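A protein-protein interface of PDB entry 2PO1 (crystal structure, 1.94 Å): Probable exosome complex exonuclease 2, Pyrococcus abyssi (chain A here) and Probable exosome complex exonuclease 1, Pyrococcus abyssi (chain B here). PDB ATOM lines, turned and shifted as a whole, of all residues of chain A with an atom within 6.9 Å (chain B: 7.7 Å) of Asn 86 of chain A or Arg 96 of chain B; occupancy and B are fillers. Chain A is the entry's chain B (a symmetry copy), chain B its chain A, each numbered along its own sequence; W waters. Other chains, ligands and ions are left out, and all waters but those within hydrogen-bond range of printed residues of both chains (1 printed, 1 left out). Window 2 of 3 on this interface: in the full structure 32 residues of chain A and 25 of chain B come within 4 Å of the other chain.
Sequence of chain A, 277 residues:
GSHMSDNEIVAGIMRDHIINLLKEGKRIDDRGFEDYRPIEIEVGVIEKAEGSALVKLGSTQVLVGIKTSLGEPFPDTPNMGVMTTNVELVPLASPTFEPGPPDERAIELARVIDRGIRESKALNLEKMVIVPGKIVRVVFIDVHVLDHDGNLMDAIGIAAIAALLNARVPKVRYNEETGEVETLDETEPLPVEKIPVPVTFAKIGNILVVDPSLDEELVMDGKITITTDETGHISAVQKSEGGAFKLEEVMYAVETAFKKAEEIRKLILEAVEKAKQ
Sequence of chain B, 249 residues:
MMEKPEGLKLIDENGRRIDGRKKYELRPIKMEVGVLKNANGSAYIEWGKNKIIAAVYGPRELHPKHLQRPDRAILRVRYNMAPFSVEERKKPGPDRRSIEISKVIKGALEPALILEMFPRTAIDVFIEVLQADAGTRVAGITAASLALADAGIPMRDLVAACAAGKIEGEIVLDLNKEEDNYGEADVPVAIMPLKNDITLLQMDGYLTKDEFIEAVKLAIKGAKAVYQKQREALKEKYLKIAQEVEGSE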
ATOM      1  N   VAL A  64      -5.161  21.967 -15.166  1.00  0.00           N
ATOM      2  CA  VAL A  64      -5.237  20.662 -14.533  1.00  0.00           C
ATOM      3  C   VAL A  64      -6.190  19.827 -15.300  1.00  0.00           C
ATOM      4  O   VAL A  64      -7.277  20.297 -15.736  1.00  0.00           O
ATOM      5  CB  VAL A  64      -5.739  20.768 -13.039  1.00  0.00           C
ATOM      6  CG1 VAL A  64      -6.042  19.366 -12.432  1.00  0.00           C
ATOM      7  CG2 VAL A  64      -4.720  21.442 -12.286  1.00  0.00           C
ATOM      8  N   THR A  84      -4.333  10.395  -7.181  1.00  0.00           N
ATOM      9  CA  THR A  84      -2.949  10.706  -7.270  1.00  0.00           C
ATOM     10  C   THR A  84      -2.740  12.045  -7.965  1.00  0.00           C
ATOM     11  O   THR A  84      -3.438  12.378  -8.927  1.00  0.00           O
ATOM     12  CB  THR A  84      -2.186   9.508  -7.966  1.00  0.00           C
ATOM     13  OG1 THR A  84      -0.806   9.798  -7.960  1.00  0.00           O
ATOM     14  CG2 THR A  84      -2.630   9.342  -9.375  1.00  0.00           C
ATOM     15  N   THR A  85      -1.815  12.839  -7.417  1.00  0.00           N
ATOM     16  CA  THR A  85      -1.593  14.200  -7.840  1.00  0.00           C
ATOM     17  C   THR A  85      -0.199  14.347  -8.305  1.00  0.00           C
ATOM     18  O   THR A  85       0.758  13.903  -7.622  1.00  0.00           O
ATOM     19  CB  THR A  85      -1.873  15.123  -6.632  1.00  0.00           C
ATOM     20  OG1 THR A  85      -3.151  14.772  -6.117  1.00  0.00           O
ATOM     21  CG2 THR A  85      -1.881  16.580  -7.023  1.00  0.00           C
ATOM     22  N   ASN A  86      -0.065  14.846  -9.532  1.00  0.00           N
ATOM     23  CA  ASN A  86       1.232  15.114 -10.104  1.00  0.00           C
ATOM     24  C   ASN A  86       1.252  16.491 -10.626  1.00  0.00           C
ATOM     25  O   ASN A  86       0.291  16.939 -11.272  1.00  0.00           O
ATOM     26  CB  ASN A  86       1.613  14.140 -11.239  1.00  0.00           C
ATOM     27  CG  ASN A  86       3.038  14.312 -11.678  1.00  0.00           C
ATOM     28  OD1 ASN A  86       3.322  14.721 -12.831  1.00  0.00           O
ATOM     29  ND2 ASN A  86       3.968  13.945 -10.808  1.00  0.00           N
ATOM     30  N   VAL A  87       2.364  17.200 -10.359  1.00  0.00           N
ATOM     31  CA  VAL A  87       2.544  18.562 -10.898  1.00  0.00           C
ATOM     32  C   VAL A  87       3.756  18.484 -11.813  1.00  0.00           C
ATOM     33  O   VAL A  87       4.829  18.051 -11.392  1.00  0.00           O
ATOM     34  CB  VAL A  87       2.854  19.489  -9.770  1.00  0.00           C
ATOM     35  CG1 VAL A  87       3.373  20.826 -10.304  1.00  0.00           C
ATOM     36  CG2 VAL A  87       1.580  19.690  -8.904  1.00  0.00           C
ATOM     37  N   GLU A  88       3.547  18.866 -13.059  1.00  0.00           N
ATOM     38  CA  GLU A  88       4.569  19.111 -14.014  1.00  0.00           C
ATOM     39  C   GLU A  88       4.831  20.611 -14.116  1.00  0.00           C
ATOM     40  O   GLU A  88       3.954  21.439 -14.471  1.00  0.00           O
ATOM     41  CB  GLU A  88       4.152  18.560 -15.355  1.00  0.00           C
ATOM     42  CG  GLU A  88       3.934  17.040 -15.348  1.00  0.00           C
ATOM     43  CD  GLU A  88       5.236  16.285 -15.129  1.00  0.00           C
ATOM     44  OE1 GLU A  88       5.353  15.500 -14.170  1.00  0.00           O
ATOM     45  OE2 GLU A  88       6.167  16.539 -15.883  1.00  0.00           O
ATOM     46  N   LEU A  89       6.039  20.954 -13.719  1.00  0.00           N
ATOM     47  CA  LEU A  89       6.581  22.329 -13.842  1.00  0.00           C
ATOM     48  C   LEU A  89       7.247  22.301 -15.207  1.00  0.00           C
ATOM     49  O   LEU A  89       8.441  22.074 -15.316  1.00  0.00           O
ATOM     50  CB  LEU A  89       7.596  22.542 -12.721  1.00  0.00           C
ATOM     51  CG  LEU A  89       7.036  23.253 -11.483  1.00  0.00           C
ATOM     52  CD1 LEU A  89       5.530  23.294 -11.251  1.00  0.00           C
ATOM     53  CD2 LEU A  89       7.803  23.008 -10.194  1.00  0.00           C
ATOM     54  N   PRO A 102       9.789  15.293 -11.551  1.00  0.00           N
ATOM     55  CA  PRO A 102       9.507  16.411 -10.644  1.00  0.00           C
ATOM     56  C   PRO A 102      10.623  16.701  -9.664  1.00  0.00           C
ATOM     57  O   PRO A 102      11.207  15.775  -9.093  1.00  0.00           O
ATOM     58  CB  PRO A 102       8.208  15.981  -9.920  1.00  0.00           C
ATOM     59  CG  PRO A 102       7.508  15.135 -10.884  1.00  0.00           C
ATOM     60  CD  PRO A 102       8.664  14.333 -11.554  1.00  0.00           C
ATOM     61  N   ALA A 106       8.027  20.797  -7.443  1.00  0.00           N
ATOM     62  CA  ALA A 106       6.862  20.182  -8.043  1.00  0.00           C
ATOM     63  C   ALA A 106       6.281  19.175  -7.050  1.00  0.00           C
ATOM     64  O   ALA A 106       5.068  19.046  -6.922  1.00  0.00           O
ATOM     65  CB  ALA A 106       7.271  19.418  -9.326  1.00  0.00           C
ATOM     66  N   ILE A 107       7.158  18.446  -6.378  1.00  0.00           N
ATOM     67  CA  ILE A 107       6.776  17.442  -5.454  1.00  0.00           C
ATOM     68  C   ILE A 107       6.070  18.063  -4.260  1.00  0.00           C
ATOM     69  O   ILE A 107       5.051  17.534  -3.830  1.00  0.00           O
ATOM     70  CB  ILE A 107       7.981  16.627  -5.007  1.00  0.00           C
ATOM     71  CG1 ILE A 107       8.378  15.730  -6.179  1.00  0.00           C
ATOM     72  CG2 ILE A 107       7.594  15.816  -3.828  1.00  0.00           C
ATOM     73  CD1 ILE A 107       9.779  15.169  -6.115  1.00  0.00           C
ATOM     74  N   GLU A 108       6.557  19.187  -3.755  1.00  0.00           N
ATOM     75  CA  GLU A 108       5.890  19.786  -2.613  1.00  0.00           C
ATOM     76  C   GLU A 108       4.534  20.357  -3.020  1.00  0.00           C
ATOM     77  O   GLU A 108       3.568  20.238  -2.282  1.00  0.00           O
ATOM     78  CB  GLU A 108       6.772  20.893  -2.002  1.00  0.00           C
ATOM     79  CG  GLU A 108       6.003  21.822  -1.025  1.00  0.00           C
ATOM     80  CD  GLU A 108       6.912  22.932  -0.541  1.00  0.00           C
ATOM     81  OE1 GLU A 108       7.210  22.970   0.655  1.00  0.00           O
ATOM     82  OE2 GLU A 108       7.420  23.696  -1.382  1.00  0.00           O
ATOM     83  N   LEU A 109       4.454  20.979  -4.195  1.00  0.00           N
ATOM     84  CA  LEU A 109       3.177  21.494  -4.710  1.00  0.00           C
ATOM     85  C   LEU A 109       2.198  20.366  -4.827  1.00  0.00           C
ATOM     86  O   LEU A 109       1.120  20.466  -4.354  1.00  0.00           O
ATOM     87  CB  LEU A 109       3.397  22.087  -6.111  1.00  0.00           C
ATOM     88  CG  LEU A 109       4.107  23.455  -6.082  1.00  0.00           C
ATOM     89  CD1 LEU A 109       4.579  23.847  -7.479  1.00  0.00           C
ATOM     90  CD2 LEU A 109       3.186  24.545  -5.510  1.00  0.00           C
ATOM     91  N   ALA A 110       2.590  19.259  -5.464  1.00  0.00           N
ATOM     92  CA  ALA A 110       1.670  18.105  -5.605  1.00  0.00           C
ATOM     93  C   ALA A 110       1.162  17.593  -4.277  1.00  0.00           C
ATOM     94  O   ALA A 110       0.033  17.161  -4.147  1.00  0.00           O
ATOM     95  CB  ALA A 110       2.372  16.967  -6.323  1.00  0.00           C
ATOM     96  N   ARG A 111       2.072  17.468  -3.333  1.00  0.00           N
ATOM     97  CA  ARG A 111       1.732  16.816  -2.105  1.00  0.00           C
ATOM     98  C   ARG A 111       0.869  17.697  -1.251  1.00  0.00           C
ATOM     99  O   ARG A 111      -0.062  17.240  -0.661  1.00  0.00           O
ATOM    100  CB  ARG A 111       3.039  16.372  -1.421  1.00  0.00           C
ATOM    101  CG  ARG A 111       3.647  15.280  -2.190  1.00  0.00           C
ATOM    102  CD  ARG A 111       4.916  14.772  -1.561  1.00  0.00           C
ATOM    103  NE  ARG A 111       4.799  14.642  -0.094  1.00  0.00           N
ATOM    104  CZ  ARG A 111       4.415  13.527   0.520  1.00  0.00           C
ATOM    105  NH1 ARG A 111       4.072  12.414  -0.177  1.00  0.00           N
ATOM    106  NH2 ARG A 111       4.393  13.507   1.839  1.00  0.00           N
ATOM    107  N   ASP A 114      -2.478  17.735  -2.856  1.00  0.00           N
ATOM    108  CA  ASP A 114      -3.105  16.458  -2.681  1.00  0.00           C
ATOM    109  C   ASP A 114      -3.648  16.392  -1.268  1.00  0.00           C
ATOM    110  O   ASP A 114      -4.763  15.922  -1.050  1.00  0.00           O
ATOM    111  CB  ASP A 114      -2.047  15.388  -2.843  1.00  0.00           C
ATOM    112  CG  ASP A 114      -2.606  14.006  -2.710  1.00  0.00           C
ATOM    113  OD1 ASP A 114      -2.826  13.352  -3.755  1.00  0.00           O
ATOM    114  OD2 ASP A 114      -2.757  13.576  -1.550  1.00  0.00           O
ATOM    115  N   PHE A 140      -6.466  10.473 -11.568  1.00  0.00           N
ATOM    116  CA  PHE A 140      -5.233  11.238 -11.764  1.00  0.00           C
ATOM    117  C   PHE A 140      -5.500  12.746 -11.869  1.00  0.00           C
ATOM    118  O   PHE A 140      -6.228  13.230 -12.765  1.00  0.00           O
ATOM    119  CB  PHE A 140      -4.489  10.767 -13.035  1.00  0.00           C
ATOM    120  CG  PHE A 140      -4.115   9.351 -13.021  1.00  0.00           C
ATOM    121  CD1 PHE A 140      -4.987   8.389 -13.498  1.00  0.00           C
ATOM    122  CD2 PHE A 140      -2.865   8.948 -12.550  1.00  0.00           C
ATOM    123  CE1 PHE A 140      -4.609   7.033 -13.495  1.00  0.00           C
ATOM    124  CE2 PHE A 140      -2.502   7.588 -12.543  1.00  0.00           C
ATOM    125  CZ  PHE A 140      -3.361   6.651 -13.024  1.00  0.00           C
ATOM    126  N   ILE A 141      -4.924  13.481 -10.934  1.00  0.00           N
ATOM    127  CA  ILE A 141      -4.975  14.898 -10.958  1.00  0.00           C
ATOM    128  C   ILE A 141      -3.641  15.298 -11.577  1.00  0.00           C
ATOM    129  O   ILE A 141      -2.587  15.138 -10.961  1.00  0.00           O
ATOM    130  CB  ILE A 141      -5.112  15.524  -9.598  1.00  0.00           C
ATOM    131  CG1 ILE A 141      -6.309  14.925  -8.873  1.00  0.00           C
ATOM    132  CG2 ILE A 141      -5.186  17.039  -9.764  1.00  0.00           C
ATOM    133  CD1 ILE A 141      -6.524  15.509  -7.513  1.00  0.00           C
ATOM    134  N   ASP A 142      -3.692  15.709 -12.840  1.00  0.00           N
ATOM    135  CA  ASP A 142      -2.446  15.983 -13.536  1.00  0.00           C
ATOM    136  C   ASP A 142      -2.379  17.492 -13.737  1.00  0.00           C
ATOM    137  O   ASP A 142      -3.272  18.123 -14.387  1.00  0.00           O
ATOM    138  CB  ASP A 142      -2.320  15.205 -14.834  1.00  0.00           C
ATOM    139  CG  ASP A 142      -1.973  13.785 -14.612  1.00  0.00           C
ATOM    140  OD1 ASP A 142      -2.772  12.920 -15.041  1.00  0.00           O
ATOM    141  OD2 ASP A 142      -0.960  13.495 -13.929  1.00  0.00           O
ATOM    142  N   VAL A 143      -1.348  18.078 -13.150  1.00  0.00           N
ATOM    143  CA  VAL A 143      -1.261  19.539 -13.063  1.00  0.00           C
ATOM    144  C   VAL A 143      -0.136  19.888 -13.993  1.00  0.00           C
ATOM    145  O   VAL A 143       1.014  19.408 -13.796  1.00  0.00           O
ATOM    146  CB  VAL A 143      -0.834  20.066 -11.707  1.00  0.00           C
ATOM    147  CG1 VAL A 143      -0.691  21.617 -11.800  1.00  0.00           C
ATOM    148  CG2 VAL A 143      -1.805  19.602 -10.568  1.00  0.00           C
ATOM    149  N   HIS A 144      -0.488  20.657 -15.024  1.00  0.00           N
ATOM    150  CA  HIS A 144       0.426  21.155 -15.985  1.00  0.00           C
ATOM    151  C   HIS A 144       0.572  22.665 -15.766  1.00  0.00           C
ATOM    152  O   HIS A 144      -0.324  23.476 -16.157  1.00  0.00           O
ATOM    153  CB  HIS A 144      -0.141  20.882 -17.379  1.00  0.00           C
ATOM    154  CG  HIS A 144       0.843  20.278 -18.312  1.00  0.00           C
ATOM    155  ND1 HIS A 144       1.461  19.081 -18.049  1.00  0.00           N
ATOM    156  CD2 HIS A 144       1.252  20.651 -19.550  1.00  0.00           C
ATOM    157  CE1 HIS A 144       2.277  18.784 -19.043  1.00  0.00           C
ATOM    158  NE2 HIS A 144       2.124  19.693 -19.987  1.00  0.00           N
ATOM    159  N   ILE A 156      -2.589  26.039  -8.482  1.00  0.00           N
ATOM    160  CA  ILE A 156      -2.703  24.614  -8.709  1.00  0.00           C
ATOM    161  C   ILE A 156      -3.839  24.038  -7.872  1.00  0.00           C
ATOM    162  O   ILE A 156      -4.602  23.227  -8.356  1.00  0.00           O
ATOM    163  CB  ILE A 156      -1.377  23.830  -8.405  1.00  0.00           C
ATOM    164  CG1 ILE A 156      -0.280  24.173  -9.418  1.00  0.00           C
ATOM    165  CG2 ILE A 156      -1.686  22.343  -8.400  1.00  0.00           C
ATOM    166  CD1 ILE A 156       1.048  23.888  -8.912  1.00  0.00           C
ATOM    167  N   LYS B  90      11.600  -0.426   2.989  1.00  0.00           N
ATOM    168  CA  LYS B  90      11.463   0.695   2.077  1.00  0.00           C
ATOM    169  C   LYS B  90      12.584   0.555   1.075  1.00  0.00           C
ATOM    170  O   LYS B  90      13.762   0.452   1.421  1.00  0.00           O
ATOM    171  CB  LYS B  90      11.628   1.967   2.889  1.00  0.00           C
ATOM    172  CG  LYS B  90      11.029   3.176   2.249  1.00  0.00           C
ATOM    173  CD  LYS B  90      11.653   4.433   2.773  1.00  0.00           C
ATOM    174  CE  LYS B  90      11.492   5.556   1.721  1.00  0.00           C
ATOM    175  NZ  LYS B  90      12.534   5.466   0.627  1.00  0.00           N
ATOM    176  N   GLY B  93      16.146   4.777  -2.217  1.00  0.00           N
ATOM    177  CA  GLY B  93      15.749   5.736  -3.257  1.00  0.00           C
ATOM    178  C   GLY B  93      15.093   6.876  -2.512  1.00  0.00           C
ATOM    179  O   GLY B  93      14.594   6.700  -1.399  1.00  0.00           O
ATOM    180  N   PRO B  94      15.226   8.103  -3.010  1.00  0.00           N
ATOM    181  CA  PRO B  94      14.216   8.922  -2.332  1.00  0.00           C
ATOM    182  C   PRO B  94      12.870   8.817  -3.035  1.00  0.00           C
ATOM    183  O   PRO B  94      12.725   8.239  -4.142  1.00  0.00           O
ATOM    184  CB  PRO B  94      14.779  10.383  -2.372  1.00  0.00           C
ATOM    185  CG  PRO B  94      16.206  10.256  -3.052  1.00  0.00           C
ATOM    186  CD  PRO B  94      16.165   8.896  -3.827  1.00  0.00           C
ATOM    187  N   ASP B  95      11.911   9.409  -2.363  1.00  0.00           N
ATOM    188  CA  ASP B  95      10.563   9.296  -2.749  1.00  0.00           C
ATOM    189  C   ASP B  95       9.956  10.634  -2.483  1.00  0.00           C
ATOM    190  O   ASP B  95      10.627  11.487  -1.931  1.00  0.00           O
ATOM    191  CB  ASP B  95       9.860   8.101  -2.030  1.00  0.00           C
ATOM    192  CG  ASP B  95       9.729   8.254  -0.501  1.00  0.00           C
ATOM    193  OD1 ASP B  95       9.159   7.334   0.099  1.00  0.00           O
ATOM    194  OD2 ASP B  95      10.165   9.200   0.126  1.00  0.00           O
ATOM    195  N   ARG B  96       8.770  10.858  -3.023  1.00  0.00           N
ATOM    196  CA  ARG B  96       8.174  12.145  -2.949  1.00  0.00           C
ATOM    197  C   ARG B  96       8.175  12.624  -1.566  1.00  0.00           C
ATOM    198  O   ARG B  96       8.509  13.746  -1.340  1.00  0.00           O
ATOM    199  CB  ARG B  96       6.768  12.122  -3.425  1.00  0.00           C
ATOM    200  CG  ARG B  96       6.627  11.185  -4.479  1.00  0.00           C
ATOM    201  CD  ARG B  96       6.477  11.872  -5.702  1.00  0.00           C
ATOM    202  NE  ARG B  96       5.226  12.587  -5.649  1.00  0.00           N
ATOM    203  CZ  ARG B  96       4.748  13.268  -6.689  1.00  0.00           C
ATOM    204  NH1 ARG B  96       5.400  13.272  -7.901  1.00  0.00           N
ATOM    205  NH2 ARG B  96       3.579  13.856  -6.536  1.00  0.00           N
ATOM    206  N   ARG B  97       7.753  11.801  -0.633  1.00  0.00           N
ATOM    207  CA  ARG B  97       7.733  12.218   0.785  1.00  0.00           C
ATOM    208  C   ARG B  97       9.104  12.614   1.281  1.00  0.00           C
ATOM    209  O   ARG B  97       9.234  13.563   1.965  1.00  0.00           O
ATOM    210  CB  ARG B  97       7.158  11.123   1.718  1.00  0.00           C
ATOM    211  CG  ARG B  97       7.227  11.463   3.255  1.00  0.00           C
ATOM    212  CD  ARG B  97       6.550  10.386   4.087  1.00  0.00           C
ATOM    213  NE  ARG B  97       6.963  10.392   5.500  1.00  0.00           N
ATOM    214  CZ  ARG B  97       8.157  10.007   5.947  1.00  0.00           C
ATOM    215  NH1 ARG B  97       9.070   9.622   5.079  1.00  0.00           N
ATOM    216  NH2 ARG B  97       8.455  10.041   7.270  1.00  0.00           N
ATOM    217  N   SER B  98      10.167  11.853   0.978  1.00  0.00           N
ATOM    218  CA  SER B  98      11.439  12.197   1.609  1.00  0.00           C
ATOM    219  C   SER B  98      12.016  13.476   0.976  1.00  0.00           C
ATOM    220  O   SER B  98      12.774  14.237   1.605  1.00  0.00           O
ATOM    221  CB  SER B  98      12.381  11.000   1.538  1.00  0.00           C
ATOM    222  OG  SER B  98      11.647   9.866   1.993  1.00  0.00           O
ATOM    223  N   ILE B  99      11.629  13.733  -0.252  1.00  0.00           N
ATOM    224  CA  ILE B  99      12.075  14.903  -0.962  1.00  0.00           C
ATOM    225  C   ILE B  99      11.318  16.083  -0.353  1.00  0.00           C
ATOM    226  O   ILE B  99      11.918  17.118  -0.119  1.00  0.00           O
ATOM    227  CB  ILE B  99      11.745  14.743  -2.408  1.00  0.00           C
ATOM    228  CG1 ILE B  99      12.781  13.796  -3.053  1.00  0.00           C
ATOM    229  CG2 ILE B  99      11.734  16.071  -3.183  1.00  0.00           C
ATOM    230  CD1 ILE B  99      12.335  13.361  -4.364  1.00  0.00           C
ATOM    231  N   GLU B 100      10.024  15.941  -0.097  1.00  0.00           N
ATOM    232  CA  GLU B 100       9.334  17.078   0.483  1.00  0.00           C
ATOM    233  C   GLU B 100       9.828  17.324   1.854  1.00  0.00           C
ATOM    234  O   GLU B 100       9.991  18.464   2.218  1.00  0.00           O
ATOM    235  CB  GLU B 100       7.797  16.940   0.481  1.00  0.00           C
ATOM    236  CG  GLU B 100       7.110  18.098   1.344  1.00  0.00           C
ATOM    237  CD  GLU B 100       5.708  17.790   1.798  1.00  0.00           C
ATOM    238  OE1 GLU B 100       5.223  16.673   1.593  1.00  0.00           O
ATOM    239  OE2 GLU B 100       5.082  18.669   2.445  1.00  0.00           O
ATOM    240  N   ILE B 101      10.059  16.282   2.639  1.00  0.00           N
ATOM    241  CA  ILE B 101      10.577  16.474   4.007  1.00  0.00           C
ATOM    242  C   ILE B 101      11.943  17.164   3.925  1.00  0.00           C
ATOM    243  O   ILE B 101      12.192  18.058   4.647  1.00  0.00           O
ATOM    244  CB  ILE B 101      10.684  15.132   4.706  1.00  0.00           C
ATOM    245  CG1 ILE B 101       9.246  14.607   4.957  1.00  0.00           C
ATOM    246  CG2 ILE B 101      11.552  15.208   6.005  1.00  0.00           C
ATOM    247  CD1 ILE B 101       9.176  13.353   5.778  1.00  0.00           C
ATOM    248  N   SER B 102      12.797  16.770   2.989  1.00  0.00           N
ATOM    249  CA  SER B 102      14.116  17.403   2.840  1.00  0.00           C
ATOM    250  C   SER B 102      13.937  18.913   2.599  1.00  0.00           C
ATOM    251  O   SER B 102      14.707  19.739   3.115  1.00  0.00           O
ATOM    252  CB  SER B 102      14.798  16.815   1.594  1.00  0.00           C
ATOM    253  OG  SER B 102      15.061  15.464   1.843  1.00  0.00           O
HETATM  254  O   HOH W   1       1.731  13.620  -4.746  1.00  0.00           O
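Of chain B, only Arg 96 (3.3 Å) comes within 4 Å of Asn 86 of chain A.
Arg 96 of chain B touches just these residues of chain A: Thr 85 (3.0 Å), Asn 86 (3.3 Å), Ile 107 (3.4 Å), Ala 110 (3.3 Å) and Arg 111 (3.7 Å).
Printed residues of chain B within 4 Å of Ala 110 of chain A: Arg 96 (3.3 Å).
Printed residues of chain B within 4 Å of Arg 111 of chain A: Arg 96 (3.7 Å), Arg 97 (3.6 Å) and Glu 100 (2.7 Å).
Of the printed residues of chain B, Ile 107 of chain A touches Arg 96 (3.4 Å) and Ile 99 (3.6 Å).
The nearest printed residue of chain B that does not touch Thr 85 of chain A is Arg 97 of chain B (10.1 Å).
The backbone NH (N) of Val 143 of chain A is in hydrogen-bond range of the backbone carbonyl oxygen (O) of Asn 86 of chain A.
The side-chain carboxylate (OD1) of Asp 114 of chain A is in hydrogen-bond range of the side-chain hydroxyl (OG1) of Thr 85 of chain A, 2.8 Å away.
The side-chain amide oxygen (OD1) of Asn 86 of chain A sits close to the side-chain carboxylate (OE1) of Glu 88 of chain A, at 2.6 Å.
The backbone NH of Asn 86 of chain A lies within hydrogen-bond range of the backbone carbonyl oxygen of Ile 141 of chain A, at 2.9 Å.
Among the printed residues, merely in contact across the chains: Ile 107 of chain A with Arg 96 of chain B, Ile 107 of chain A with Ile 99 of chain B, Ala 110 of chain A with Arg 96 of chain B, Arg 111 of chain A with Arg 96 of chain B and Arg 111 of chain A with Arg 97 of chain B.
Of the 11 printed residues of chain B, 4 touch a printed residue of chain A.
Printed residues of chain B that touch a printed residue of chain A: Arg 96, Arg 97, Ile 99 and Glu 100.
Printed residues of chain A that touch a printed residue of chain B: Thr 85, Asn 86, Ile 107, Ala 110 and Arg 111.
Hydrophobic or aromatic side chains of chain A within 4 Å of the printed part of chain B: Ile 107 and Ala 110.
Among the printed residues, Asp or Glu carboxylates within 4 Å of a Lys or Arg side-chain nitrogen of the other chain: Arg 111 of chain A with Glu 100 of chain B (2.7 Å).
Water W1 bridges the guanidinium group (NH2) of Arg 96 of chain B (2.6 Å) and the backbone carbonyl oxygen (O) of Thr 85 of chain A (3.0 Å).
OE1 of Glu 100 of chain B lies within salt-bridge range of NE of Arg 111 of chain A, 2.7 Å away.
The guanidinium group (NH1) of Arg 96 of chain B sits close to the side-chain amide nitrogen (ND2) of Asn 86 of chain A.
NH2 of Arg 96 of chain B lies within hydrogen-bond range of O of Thr 85 of chain A, at 3.0 Å.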
